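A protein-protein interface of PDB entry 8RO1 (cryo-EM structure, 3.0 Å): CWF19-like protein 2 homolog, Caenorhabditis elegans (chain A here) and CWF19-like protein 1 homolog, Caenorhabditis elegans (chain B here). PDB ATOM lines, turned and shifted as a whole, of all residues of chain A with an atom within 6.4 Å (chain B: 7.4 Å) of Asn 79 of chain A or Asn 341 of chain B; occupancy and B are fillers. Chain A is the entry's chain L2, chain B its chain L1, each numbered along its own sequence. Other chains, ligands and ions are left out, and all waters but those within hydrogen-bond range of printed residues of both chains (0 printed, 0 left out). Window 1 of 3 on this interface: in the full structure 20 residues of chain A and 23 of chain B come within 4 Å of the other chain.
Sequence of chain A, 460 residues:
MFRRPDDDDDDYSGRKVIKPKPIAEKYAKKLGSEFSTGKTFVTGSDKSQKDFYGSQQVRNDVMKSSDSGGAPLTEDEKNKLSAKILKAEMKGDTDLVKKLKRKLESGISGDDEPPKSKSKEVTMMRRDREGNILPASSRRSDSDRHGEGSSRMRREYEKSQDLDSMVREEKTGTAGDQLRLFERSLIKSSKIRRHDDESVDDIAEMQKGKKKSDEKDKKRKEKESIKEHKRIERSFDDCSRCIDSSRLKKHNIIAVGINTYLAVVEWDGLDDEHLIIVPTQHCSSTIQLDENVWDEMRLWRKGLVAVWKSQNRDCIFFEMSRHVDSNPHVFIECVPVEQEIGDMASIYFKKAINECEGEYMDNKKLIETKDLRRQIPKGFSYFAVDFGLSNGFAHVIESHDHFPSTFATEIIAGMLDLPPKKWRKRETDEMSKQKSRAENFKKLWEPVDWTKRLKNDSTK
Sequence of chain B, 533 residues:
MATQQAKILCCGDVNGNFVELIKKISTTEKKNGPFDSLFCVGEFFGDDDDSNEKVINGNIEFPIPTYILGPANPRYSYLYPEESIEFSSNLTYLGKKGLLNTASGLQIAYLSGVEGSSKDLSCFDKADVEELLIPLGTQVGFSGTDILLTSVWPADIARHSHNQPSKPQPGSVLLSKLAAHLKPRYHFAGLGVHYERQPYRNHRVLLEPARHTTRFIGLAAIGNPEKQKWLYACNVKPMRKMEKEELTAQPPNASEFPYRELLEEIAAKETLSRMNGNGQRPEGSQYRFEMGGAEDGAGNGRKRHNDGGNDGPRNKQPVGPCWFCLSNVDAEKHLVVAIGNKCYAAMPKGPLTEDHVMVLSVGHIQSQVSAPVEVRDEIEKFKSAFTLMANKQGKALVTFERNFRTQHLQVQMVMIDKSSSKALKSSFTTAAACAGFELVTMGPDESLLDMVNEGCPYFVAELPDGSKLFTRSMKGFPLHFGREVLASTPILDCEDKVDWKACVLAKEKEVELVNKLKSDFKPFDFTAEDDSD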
ATOM      1  N   GLU A  75     -23.157  16.651 -26.108  1.00  0.00           N
ATOM      2  CA  GLU A  75     -21.804  17.158 -25.911  1.00  0.00           C
ATOM      3  C   GLU A  75     -21.805  18.487 -25.168  1.00  0.00           C
ATOM      4  O   GLU A  75     -21.005  18.680 -24.256  1.00  0.00           O
ATOM      5  CB  GLU A  75     -21.086  17.322 -27.252  1.00  0.00           C
ATOM      6  CG  GLU A  75     -19.617  17.704 -27.115  1.00  0.00           C
ATOM      7  CD  GLU A  75     -18.835  17.501 -28.397  1.00  0.00           C
ATOM      8  OE1 GLU A  75     -19.408  17.715 -29.486  1.00  0.00           O
ATOM      9  OE2 GLU A  75     -17.643  17.134 -28.315  1.00  0.00           O
ATOM     10  N   ASP A  76     -22.699  19.392 -25.590  1.00  0.00           N
ATOM     11  CA  ASP A  76     -22.641  20.801 -25.182  1.00  0.00           C
ATOM     12  C   ASP A  76     -22.619  20.998 -23.670  1.00  0.00           C
ATOM     13  O   ASP A  76     -22.126  22.022 -23.192  1.00  0.00           O
ATOM     14  CB  ASP A  76     -23.810  21.594 -25.783  1.00  0.00           C
ATOM     15  CG  ASP A  76     -23.953  21.395 -27.283  1.00  0.00           C
ATOM     16  OD1 ASP A  76     -23.613  20.298 -27.773  1.00  0.00           O
ATOM     17  OD2 ASP A  76     -24.399  22.339 -27.970  1.00  0.00           O
ATOM     18  N   GLU A  77     -23.167  20.056 -22.898  1.00  0.00           N
ATOM     19  CA  GLU A  77     -23.061  20.162 -21.446  1.00  0.00           C
ATOM     20  C   GLU A  77     -21.611  20.105 -20.970  1.00  0.00           C
ATOM     21  O   GLU A  77     -21.294  20.631 -19.897  1.00  0.00           O
ATOM     22  CB  GLU A  77     -23.880  19.056 -20.782  1.00  0.00           C
ATOM     23  CG  GLU A  77     -25.365  19.134 -21.089  1.00  0.00           C
ATOM     24  CD  GLU A  77     -26.219  18.581 -19.968  1.00  0.00           C
ATOM     25  OE1 GLU A  77     -26.112  17.371 -19.681  1.00  0.00           O
ATOM     26  OE2 GLU A  77     -26.994  19.358 -19.370  1.00  0.00           O
ATOM     27  N   LYS A  78     -20.720  19.475 -21.744  1.00  0.00           N
ATOM     28  CA  LYS A  78     -19.290  19.556 -21.456  1.00  0.00           C
ATOM     29  C   LYS A  78     -18.769  20.986 -21.523  1.00  0.00           C
ATOM     30  O   LYS A  78     -17.773  21.314 -20.868  1.00  0.00           O
ATOM     31  CB  LYS A  78     -18.505  18.685 -22.436  1.00  0.00           C
ATOM     32  CG  LYS A  78     -18.738  17.195 -22.275  1.00  0.00           C
ATOM     33  CD  LYS A  78     -17.766  16.392 -23.121  1.00  0.00           C
ATOM     34  CE  LYS A  78     -17.993  14.899 -22.963  1.00  0.00           C
ATOM     35  NZ  LYS A  78     -16.999  14.100 -23.729  1.00  0.00           N
ATOM     36  N   ASN A  79     -19.422  21.852 -22.306  1.00  0.00           N
ATOM     37  CA  ASN A  79     -18.992  23.243 -22.381  1.00  0.00           C
ATOM     38  C   ASN A  79     -19.285  23.999 -21.094  1.00  0.00           C
ATOM     39  O   ASN A  79     -18.529  24.906 -20.726  1.00  0.00           O
ATOM     40  CB  ASN A  79     -19.696  23.936 -23.546  1.00  0.00           C
ATOM     41  CG  ASN A  79     -19.421  23.264 -24.873  1.00  0.00           C
ATOM     42  OD1 ASN A  79     -18.401  22.598 -25.048  1.00  0.00           O
ATOM     43  ND2 ASN A  79     -20.345  23.418 -25.813  1.00  0.00           N
ATOM     44  N   LYS A  80     -20.372  23.650 -20.407  1.00  0.00           N
ATOM     45  CA  LYS A  80     -20.646  24.253 -19.107  1.00  0.00           C
ATOM     46  C   LYS A  80     -19.559  23.913 -18.093  1.00  0.00           C
ATOM     47  O   LYS A  80     -18.947  24.807 -17.498  1.00  0.00           O
ATOM     48  CB  LYS A  80     -22.012  23.790 -18.584  1.00  0.00           C
ATOM     49  CG  LYS A  80     -23.043  24.895 -18.448  1.00  0.00           C
ATOM     50  CD  LYS A  80     -24.399  24.328 -18.048  1.00  0.00           C
ATOM     51  CE  LYS A  80     -25.463  25.412 -17.971  1.00  0.00           C
ATOM     52  NZ  LYS A  80     -26.784  24.873 -17.545  1.00  0.00           N
ATOM     53  N   LEU A  81     -19.267  22.622 -17.926  1.00  0.00           N
ATOM     54  CA  LEU A  81     -18.328  22.197 -16.890  1.00  0.00           C
ATOM     55  C   LEU A  81     -16.900  22.641 -17.187  1.00  0.00           C
ATOM     56  O   LEU A  81     -16.153  22.995 -16.267  1.00  0.00           O
ATOM     57  CB  LEU A  81     -18.394  20.679 -16.741  1.00  0.00           C
ATOM     58  CG  LEU A  81     -19.746  20.108 -16.300  1.00  0.00           C
ATOM     59  CD1 LEU A  81     -19.713  18.587 -16.335  1.00  0.00           C
ATOM     60  CD2 LEU A  81     -20.155  20.613 -14.926  1.00  0.00           C
ATOM     61  N   SER A  82     -16.498  22.607 -18.459  1.00  0.00           N
ATOM     62  CA  SER A  82     -15.208  23.167 -18.857  1.00  0.00           C
ATOM     63  C   SER A  82     -15.109  24.642 -18.495  1.00  0.00           C
ATOM     64  O   SER A  82     -14.041  25.130 -18.106  1.00  0.00           O
ATOM     65  CB  SER A  82     -14.996  22.978 -20.359  1.00  0.00           C
ATOM     66  OG  SER A  82     -14.930  21.605 -20.698  1.00  0.00           O
ATOM     67  N   ALA A  83     -16.219  25.364 -18.620  1.00  0.00           N
ATOM     68  CA  ALA A  83     -16.269  26.788 -18.319  1.00  0.00           C
ATOM     69  C   ALA A  83     -16.363  27.074 -16.817  1.00  0.00           C
ATOM     70  O   ALA A  83     -15.722  28.005 -16.318  1.00  0.00           O
ATOM     71  CB  ALA A  83     -17.461  27.375 -19.080  1.00  0.00           C
ATOM     72  N   LYS A  84     -17.127  26.271 -16.080  1.00  0.00           N
ATOM     73  CA  LYS A  84     -17.304  26.444 -14.636  1.00  0.00           C
ATOM     74  C   LYS A  84     -16.025  26.384 -13.790  1.00  0.00           C
ATOM     75  O   LYS A  84     -16.062  26.816 -12.632  1.00  0.00           O
ATOM     76  CB  LYS A  84     -18.286  25.397 -14.103  1.00  0.00           C
ATOM     77  CG  LYS A  84     -19.748  25.675 -14.433  1.00  0.00           C
ATOM     78  CD  LYS A  84     -20.674  24.687 -13.741  1.00  0.00           C
ATOM     79  CE  LYS A  84     -22.133  24.994 -14.036  1.00  0.00           C
ATOM     80  NZ  LYS A  84     -23.056  24.114 -13.267  1.00  0.00           N
ATOM     81  N   LYS A  87     -15.002  29.800 -13.148  1.00  0.00           N
ATOM     82  CA  LYS A  87     -16.194  30.388 -12.544  1.00  0.00           C
ATOM     83  C   LYS A  87     -16.227  30.185 -11.036  1.00  0.00           C
ATOM     84  O   LYS A  87     -16.603  31.098 -10.290  1.00  0.00           O
ATOM     85  CB  LYS A  87     -17.409  29.720 -13.183  1.00  0.00           C
ATOM     86  CG  LYS A  87     -18.701  30.455 -13.246  1.00  0.00           C
ATOM     87  CD  LYS A  87     -19.720  29.482 -13.840  1.00  0.00           C
ATOM     88  CE  LYS A  87     -21.043  30.115 -14.060  1.00  0.00           C
ATOM     89  NZ  LYS A  87     -21.713  30.498 -12.800  1.00  0.00           N
ATOM     90  N   ILE B 339     -16.001  33.719 -17.639  1.00  0.00           N
ATOM     91  CA  ILE B 339     -16.188  32.342 -18.084  1.00  0.00           C
ATOM     92  C   ILE B 339     -17.452  31.852 -17.382  1.00  0.00           C
ATOM     93  O   ILE B 339     -17.372  31.175 -16.351  1.00  0.00           O
ATOM     94  CB  ILE B 339     -14.960  31.440 -17.804  1.00  0.00           C
ATOM     95  CG1 ILE B 339     -13.687  32.022 -18.441  1.00  0.00           C
ATOM     96  CG2 ILE B 339     -15.150  30.038 -18.387  1.00  0.00           C
ATOM     97  CD1 ILE B 339     -12.421  31.151 -18.319  1.00  0.00           C
ATOM     98  N   GLY B 340     -18.623  32.180 -17.932  1.00  0.00           N
ATOM     99  CA  GLY B 340     -19.863  31.735 -17.326  1.00  0.00           C
ATOM    100  C   GLY B 340     -20.205  30.296 -17.662  1.00  0.00           C
ATOM    101  O   GLY B 340     -19.323  29.438 -17.621  1.00  0.00           O
ATOM    102  N   ASN B 341     -21.472  30.009 -17.972  1.00  0.00           N
ATOM    103  CA  ASN B 341     -21.898  28.636 -18.234  1.00  0.00           C
ATOM    104  C   ASN B 341     -21.649  28.239 -19.691  1.00  0.00           C
ATOM    105  O   ASN B 341     -20.549  27.790 -20.034  1.00  0.00           O
ATOM    106  CB  ASN B 341     -23.375  28.438 -17.844  1.00  0.00           C
ATOM    107  CG  ASN B 341     -23.577  28.220 -16.355  1.00  0.00           C
ATOM    108  OD1 ASN B 341     -22.727  27.651 -15.673  1.00  0.00           O
ATOM    109  ND2 ASN B 341     -24.715  28.676 -15.844  1.00  0.00           N
ATOM    110  N   LYS B 342     -22.658  28.399 -20.556  1.00  0.00           N
ATOM    111  CA  LYS B 342     -22.525  28.057 -21.967  1.00  0.00           C
ATOM    112  C   LYS B 342     -21.505  28.908 -22.713  1.00  0.00           C
ATOM    113  O   LYS B 342     -21.058  28.494 -23.789  1.00  0.00           O
ATOM    114  CB  LYS B 342     -23.888  28.173 -22.660  1.00  0.00           C
ATOM    115  CG  LYS B 342     -24.809  26.962 -22.490  1.00  0.00           C
ATOM    116  CD  LYS B 342     -24.341  25.720 -23.288  1.00  0.00           C
ATOM    117  CE  LYS B 342     -25.079  24.417 -22.927  1.00  0.00           C
ATOM    118  NZ  LYS B 342     -25.549  24.271 -21.519  1.00  0.00           N
ATOM    119  N   CYS B 343     -21.123  30.070 -22.179  1.00  0.00           N
ATOM    120  CA  CYS B 343     -20.296  31.020 -22.908  1.00  0.00           C
ATOM    121  C   CYS B 343     -19.277  31.666 -21.995  1.00  0.00           C
ATOM    122  O   CYS B 343     -19.470  31.758 -20.779  1.00  0.00           O
ATOM    123  CB  CYS B 343     -21.124  32.157 -23.504  1.00  0.00           C
ATOM    124  SG  CYS B 343     -22.364  31.650 -24.648  1.00  0.00           S
ATOM    125  N   TYR B 344     -18.182  32.104 -22.611  1.00  0.00           N
ATOM    126  CA  TYR B 344     -17.101  32.778 -21.918  1.00  0.00           C
ATOM    127  C   TYR B 344     -16.776  34.066 -22.655  1.00  0.00           C
ATOM    128  O   TYR B 344     -16.851  34.140 -23.885  1.00  0.00           O
ATOM    129  CB  TYR B 344     -15.859  31.887 -21.823  1.00  0.00           C
ATOM    130  CG  TYR B 344     -15.024  31.813 -23.081  1.00  0.00           C
ATOM    131  CD1 TYR B 344     -15.443  31.071 -24.171  1.00  0.00           C
ATOM    132  CD2 TYR B 344     -13.806  32.467 -23.168  1.00  0.00           C
ATOM    133  CE1 TYR B 344     -14.682  30.989 -25.317  1.00  0.00           C
ATOM    134  CE2 TYR B 344     -13.035  32.394 -24.312  1.00  0.00           C
ATOM    135  CZ  TYR B 344     -13.479  31.655 -25.386  1.00  0.00           C
ATOM    136  OH  TYR B 344     -12.716  31.573 -26.528  1.00  0.00           O
ATOM    137  N   SER B 361     -18.364  30.857 -27.857  1.00  0.00           N
ATOM    138  CA  SER B 361     -18.914  29.609 -27.345  1.00  0.00           C
ATOM    139  C   SER B 361     -17.816  28.560 -27.210  1.00  0.00           C
ATOM    140  O   SER B 361     -16.958  28.423 -28.086  1.00  0.00           O
ATOM    141  CB  SER B 361     -20.024  29.096 -28.265  1.00  0.00           C
ATOM    142  OG  SER B 361     -19.538  28.840 -29.572  1.00  0.00           O
ATOM    143  N   VAL B 362     -17.855  27.810 -26.108  1.00  0.00           N
ATOM    144  CA  VAL B 362     -16.757  26.897 -25.793  1.00  0.00           C
ATOM    145  C   VAL B 362     -16.846  25.677 -26.700  1.00  0.00           C
ATOM    146  O   VAL B 362     -15.820  25.082 -27.049  1.00  0.00           O
ATOM    147  CB  VAL B 362     -16.762  26.494 -24.303  1.00  0.00           C
ATOM    148  CG1 VAL B 362     -15.623  25.499 -23.971  1.00  0.00           C
ATOM    149  CG2 VAL B 362     -16.694  27.719 -23.397  1.00  0.00           C
ATOM    150  N   GLY B 363     -18.060  25.289 -27.087  1.00  0.00           N
ATOM    151  CA  GLY B 363     -18.225  24.380 -28.201  1.00  0.00           C
ATOM    152  C   GLY B 363     -18.095  25.089 -29.536  1.00  0.00           C
ATOM    153  O   GLY B 363     -18.375  26.279 -29.677  1.00  0.00           O
ATOM    154  N   HIS B 364     -17.652  24.325 -30.528  1.00  0.00           N
ATOM    155  CA  HIS B 364     -17.359  24.837 -31.864  1.00  0.00           C
ATOM    156  C   HIS B 364     -18.656  25.049 -32.637  1.00  0.00           C
ATOM    157  O   HIS B 364     -19.225  24.106 -33.192  1.00  0.00           O
ATOM    158  CB  HIS B 364     -16.432  23.871 -32.593  1.00  0.00           C
ATOM    159  CG  HIS B 364     -15.835  24.435 -33.842  1.00  0.00           C
ATOM    160  ND1 HIS B 364     -14.929  25.473 -33.828  1.00  0.00           N
ATOM    161  CD2 HIS B 364     -16.008  24.104 -35.143  1.00  0.00           C
ATOM    162  CE1 HIS B 364     -14.569  25.757 -35.067  1.00  0.00           C
ATOM    163  NE2 HIS B 364     -15.212  24.942 -35.883  1.00  0.00           N
ATOM    164  N   ILE B 365     -19.125  26.299 -32.669  1.00  0.00           N
ATOM    165  CA  ILE B 365     -20.437  26.666 -33.196  1.00  0.00           C
ATOM    166  C   ILE B 365     -20.214  27.762 -34.229  1.00  0.00           C
ATOM    167  O   ILE B 365     -19.353  28.629 -34.049  1.00  0.00           O
ATOM    168  CB  ILE B 365     -21.407  27.132 -32.080  1.00  0.00           C
ATOM    169  CG1 ILE B 365     -21.590  26.035 -31.015  1.00  0.00           C
ATOM    170  CG2 ILE B 365     -22.797  27.511 -32.647  1.00  0.00           C
ATOM    171  CD1 ILE B 365     -22.283  26.500 -29.748  1.00  0.00           C
ATOM    172  N   PRO B 372     -27.458  26.703 -29.646  1.00  0.00           N
ATOM    173  CA  PRO B 372     -28.646  26.471 -28.812  1.00  0.00           C
ATOM    174  C   PRO B 372     -29.152  27.725 -28.105  1.00  0.00           C
ATOM    175  O   PRO B 372     -28.466  28.744 -27.994  1.00  0.00           O
ATOM    176  CB  PRO B 372     -28.174  25.420 -27.800  1.00  0.00           C
ATOM    177  CG  PRO B 372     -27.070  24.721 -28.471  1.00  0.00           C
ATOM    178  CD  PRO B 372     -26.382  25.750 -29.302  1.00  0.00           C
ATOM    179  N   GLU B 374     -29.689  28.145 -24.964  1.00  0.00           N
ATOM    180  CA  GLU B 374     -28.923  28.473 -23.765  1.00  0.00           C
ATOM    181  C   GLU B 374     -27.677  29.276 -24.100  1.00  0.00           C
ATOM    182  O   GLU B 374     -27.263  30.132 -23.309  1.00  0.00           O
ATOM    183  CB  GLU B 374     -28.535  27.200 -23.012  1.00  0.00           C
ATOM    184  CG  GLU B 374     -29.709  26.390 -22.484  1.00  0.00           C
ATOM    185  CD  GLU B 374     -29.289  25.034 -21.949  1.00  0.00           C
ATOM    186  OE1 GLU B 374     -28.072  24.744 -21.936  1.00  0.00           O
ATOM    187  OE2 GLU B 374     -30.175  24.254 -21.541  1.00  0.00           O
ATOM    188  N   VAL B 375     -27.067  29.022 -25.255  1.00  0.00           N
ATOM    189  CA  VAL B 375     -25.914  29.815 -25.664  1.00  0.00           C
ATOM    190  C   VAL B 375     -26.364  31.229 -26.012  1.00  0.00           C
ATOM    191  O   VAL B 375     -25.770  32.215 -25.563  1.00  0.00           O
ATOM    192  CB  VAL B 375     -25.200  29.136 -26.852  1.00  0.00           C
ATOM    193  CG1 VAL B 375     -24.069  30.006 -27.440  1.00  0.00           C
ATOM    194  CG2 VAL B 375     -24.627  27.774 -26.448  1.00  0.00           C
ATOM    195  N   GLU B 378     -27.333  33.160 -22.798  1.00  0.00           N
ATOM    196  CA  GLU B 378     -26.218  33.705 -22.031  1.00  0.00           C
ATOM    197  C   GLU B 378     -25.570  34.885 -22.739  1.00  0.00           C
ATOM    198  O   GLU B 378     -25.047  35.791 -22.079  1.00  0.00           O
ATOM    199  CB  GLU B 378     -25.167  32.631 -21.756  1.00  0.00           C
ATOM    200  CG  GLU B 378     -24.263  32.989 -20.587  1.00  0.00           C
ATOM    201  CD  GLU B 378     -23.480  31.814 -20.059  1.00  0.00           C
ATOM    202  OE1 GLU B 378     -22.750  31.180 -20.846  1.00  0.00           O
ATOM    203  OE2 GLU B 378     -23.573  31.549 -18.845  1.00  0.00           O
ATOM    204  N   LYS B 381     -27.565  37.564 -21.736  1.00  0.00           N
ATOM    205  CA  LYS B 381     -27.218  37.877 -20.351  1.00  0.00           C
ATOM    206  C   LYS B 381     -25.915  38.665 -20.263  1.00  0.00           C
ATOM    207  O   LYS B 381     -25.809  39.613 -19.476  1.00  0.00           O
ATOM    208  CB  LYS B 381     -27.107  36.597 -19.534  1.00  0.00           C
ATOM    209  CG  LYS B 381     -28.433  35.945 -19.187  1.00  0.00           C
ATOM    210  CD  LYS B 381     -28.224  34.726 -18.304  1.00  0.00           C
ATOM    211  CE  LYS B 381     -29.532  34.011 -18.015  1.00  0.00           C
ATOM    212  NZ  LYS B 381     -29.309  32.796 -17.184  1.00  0.00           N
ATOM    213  N   PHE B 382     -24.910  38.274 -21.049  1.00  0.00           N
ATOM    214  CA  PHE B 382     -23.657  39.022 -21.100  1.00  0.00           C
ATOM    215  C   PHE B 382     -23.888  40.452 -21.573  1.00  0.00           C
ATOM    216  O   PHE B 382     -23.273  41.390 -21.051  1.00  0.00           O
ATOM    217  CB  PHE B 382     -22.650  38.313 -22.011  1.00  0.00           C
ATOM    218  CG  PHE B 382     -21.790  37.292 -21.306  1.00  0.00           C
ATOM    219  CD1 PHE B 382     -20.861  37.679 -20.352  1.00  0.00           C
ATOM    220  CD2 PHE B 382     -21.898  35.946 -21.613  1.00  0.00           C
ATOM    221  CE1 PHE B 382     -20.069  36.745 -19.712  1.00  0.00           C
ATOM    222  CE2 PHE B 382     -21.107  35.007 -20.977  1.00  0.00           C
ATOM    223  CZ  PHE B 382     -20.195  35.407 -20.024  1.00  0.00           C
ATOM    224  N   PHE B 526     -22.861  38.106 -12.014  1.00  0.00           N
ATOM    225  CA  PHE B 526     -23.875  37.295 -11.351  1.00  0.00           C
ATOM    226  C   PHE B 526     -23.583  35.805 -11.460  1.00  0.00           C
ATOM    227  O   PHE B 526     -24.207  35.010 -10.750  1.00  0.00           O
ATOM    228  CB  PHE B 526     -25.268  37.549 -11.961  1.00  0.00           C
ATOM    229  CG  PHE B 526     -25.386  37.157 -13.424  1.00  0.00           C
ATOM    230  CD1 PHE B 526     -25.055  38.041 -14.441  1.00  0.00           C
ATOM    231  CD2 PHE B 526     -25.862  35.899 -13.774  1.00  0.00           C
ATOM    232  CE1 PHE B 526     -25.163  37.666 -15.765  1.00  0.00           C
ATOM    233  CE2 PHE B 526     -25.971  35.522 -15.090  1.00  0.00           C
ATOM    234  CZ  PHE B 526     -25.623  36.402 -16.085  1.00  0.00           C
ATOM    235  N   THR B 527     -22.649  35.418 -12.332  1.00  0.00           N
ATOM    236  CA  THR B 527     -22.309  34.014 -12.514  1.00  0.00           C
ATOM    237  C   THR B 527     -21.471  33.485 -11.357  1.00  0.00           C
ATOM    238  O   THR B 527     -21.502  32.283 -11.068  1.00  0.00           O
ATOM    239  CB  THR B 527     -21.580  33.809 -13.845  1.00  0.00           C
ATOM    240  OG1 THR B 527     -20.203  34.187 -13.723  1.00  0.00           O
ATOM    241  CG2 THR B 527     -22.242  34.586 -14.993  1.00  0.00           C
ATOM    242  N   ASP B 530     -23.684  31.490  -9.030  1.00  0.00           N
ATOM    243  CA  ASP B 530     -24.477  30.373  -9.535  1.00  0.00           C
ATOM    244  C   ASP B 530     -23.822  29.020  -9.265  1.00  0.00           C
ATOM    245  O   ASP B 530     -24.473  27.986  -9.452  1.00  0.00           O
ATOM    246  CB  ASP B 530     -24.725  30.535 -11.039  1.00  0.00           C
ATOM    247  CG  ASP B 530     -25.830  31.537 -11.363  1.00  0.00           C
ATOM    248  OD1 ASP B 530     -26.699  31.806 -10.506  1.00  0.00           O
ATOM    249  OD2 ASP B 530     -25.826  32.062 -12.496  1.00  0.00           O
ATOM    250  N   ASP B 531     -22.556  29.004  -8.835  1.00  0.00           N
ATOM    251  CA  ASP B 531     -21.757  27.789  -8.710  1.00  0.00           C
ATOM    252  C   ASP B 531     -22.189  26.877  -7.569  1.00  0.00           C
ATOM    253  O   ASP B 531     -21.644  25.772  -7.459  1.00  0.00           O
ATOM    254  CB  ASP B 531     -20.288  28.162  -8.518  1.00  0.00           C
ATOM    255  CG  ASP B 531     -19.733  28.943  -9.684  1.00  0.00           C
ATOM    256  OD1 ASP B 531     -20.275  28.809 -10.798  1.00  0.00           O
ATOM    257  OD2 ASP B 531     -18.765  29.704  -9.484  1.00  0.00           O
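The side-chain amide nitrogen (ND2) of Asn 79 of chain A lies close to the backbone NH (N) of Gly 363 of chain B, at 3.2 Å.
The backbone carbonyl oxygen (O) of Thr 527 of chain B sits at hydrogen-bond distance from the side-chain amino group (NZ) of Lys 87 of chain A.
The side-chain carboxylate (OD1) of Asp 531 of chain B lies within salt-bridge range of the side-chain amino group (NZ) of Lys 87 of chain A (3.0 Å).
N of Asn 341 of chain B is in hydrogen-bond range of OE2 of Glu 378 of chain B (2.7 Å).
NZ of Lys 342 of chain B is in salt-bridge range of OE1 of Glu 374 of chain B, 2.6 Å away.
The side-chain carboxylate (OE1) of Glu 378 of chain B is in hydrogen-bond range of the backbone NH (N) of Lys 342 of chain B, at 2.8 Å.
OG of Ser 361 of chain B lies within hydrogen-bond range of O of Gly 363 of chain B, 2.8 Å away.
The side-chain amide nitrogen (ND2) of Asn 79 of chain A lies close to the backbone carbonyl oxygen (O) of Asp 76 of chain A (3.5 Å).
CE of Lys 342 of chain B touches O of Asp 76 of chain A (3.8 Å).
OD2 of Asp 76 of chain A touches CG of Pro 372 of chain B (3.6 Å).
Asn 341 of chain B touches Asn 79 of chain A.
Val 362 of chain B touches Asn 79 of chain A (C to OD1, 3.8 Å).
Lys 80 of chain A touches Asn 341 of chain B (CG to CB, 3.6 Å).
O of Ala 83 of chain A touches CG2 of Ile 339 of chain B, at 3.0 Å.
O of Gly 340 of chain B touches CB of Ala 83 of chain A, 3.1 Å away.
CB of Ala 83 of chain A touches O of Asn 341 of chain B (3.3 Å).
Lys 87 of chain A touches Ile 339 of chain B.
CE of Lys 87 of chain A touches C of Gly 340 of chain B, at 3.7 Å.
Asn 79 of chain A touches just these residues of chain B: Asn 341, Val 362 and Gly 363.
Leu 81 of chain A touches none of the printed residues of chain B.
Printed residues of chain A within 4 Å of Gly 340 of chain B: Ala 83 (3.1 Å) and Lys 87 (3.7 Å).
Of the printed residues of chain A, Asn 341 of chain B touches Asn 79 (3.6 Å), Lys 80 (3.6 Å), Ala 83 (3.3 Å), Lys 84 (3.2 Å) and Lys 87 (3.4 Å).
Printed residues of chain A within 4 Å of Thr 527 of chain B: Lys 87 (2.5 Å).
Of the printed residues of chain A, Asp 530 of chain B touches Lys 87.
Of the printed residues of chain A, Asp 531 of chain B touches Lys 87 (2.7 Å).
The nearest printed residue of chain B that does not touch Lys 87 of chain A is Phe 526 of chain B (5.5 Å).
Of the 11 printed residues of chain A, 6 touch a printed residue of chain B.
Of the 21 printed residues of chain B, 10 touch a printed residue of chain A.
Printed residues of chain B that touch a printed residue of chain A: Ile 339, Gly 340, Asn 341, Lys 342, Val 362, Gly 363, Pro 372, Thr 527, Asp 530 and Asp 531.
Hydrophobic or aromatic side chains of chain B that line the printed part of chain A: Ile 339, Val 362 and Pro 372.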
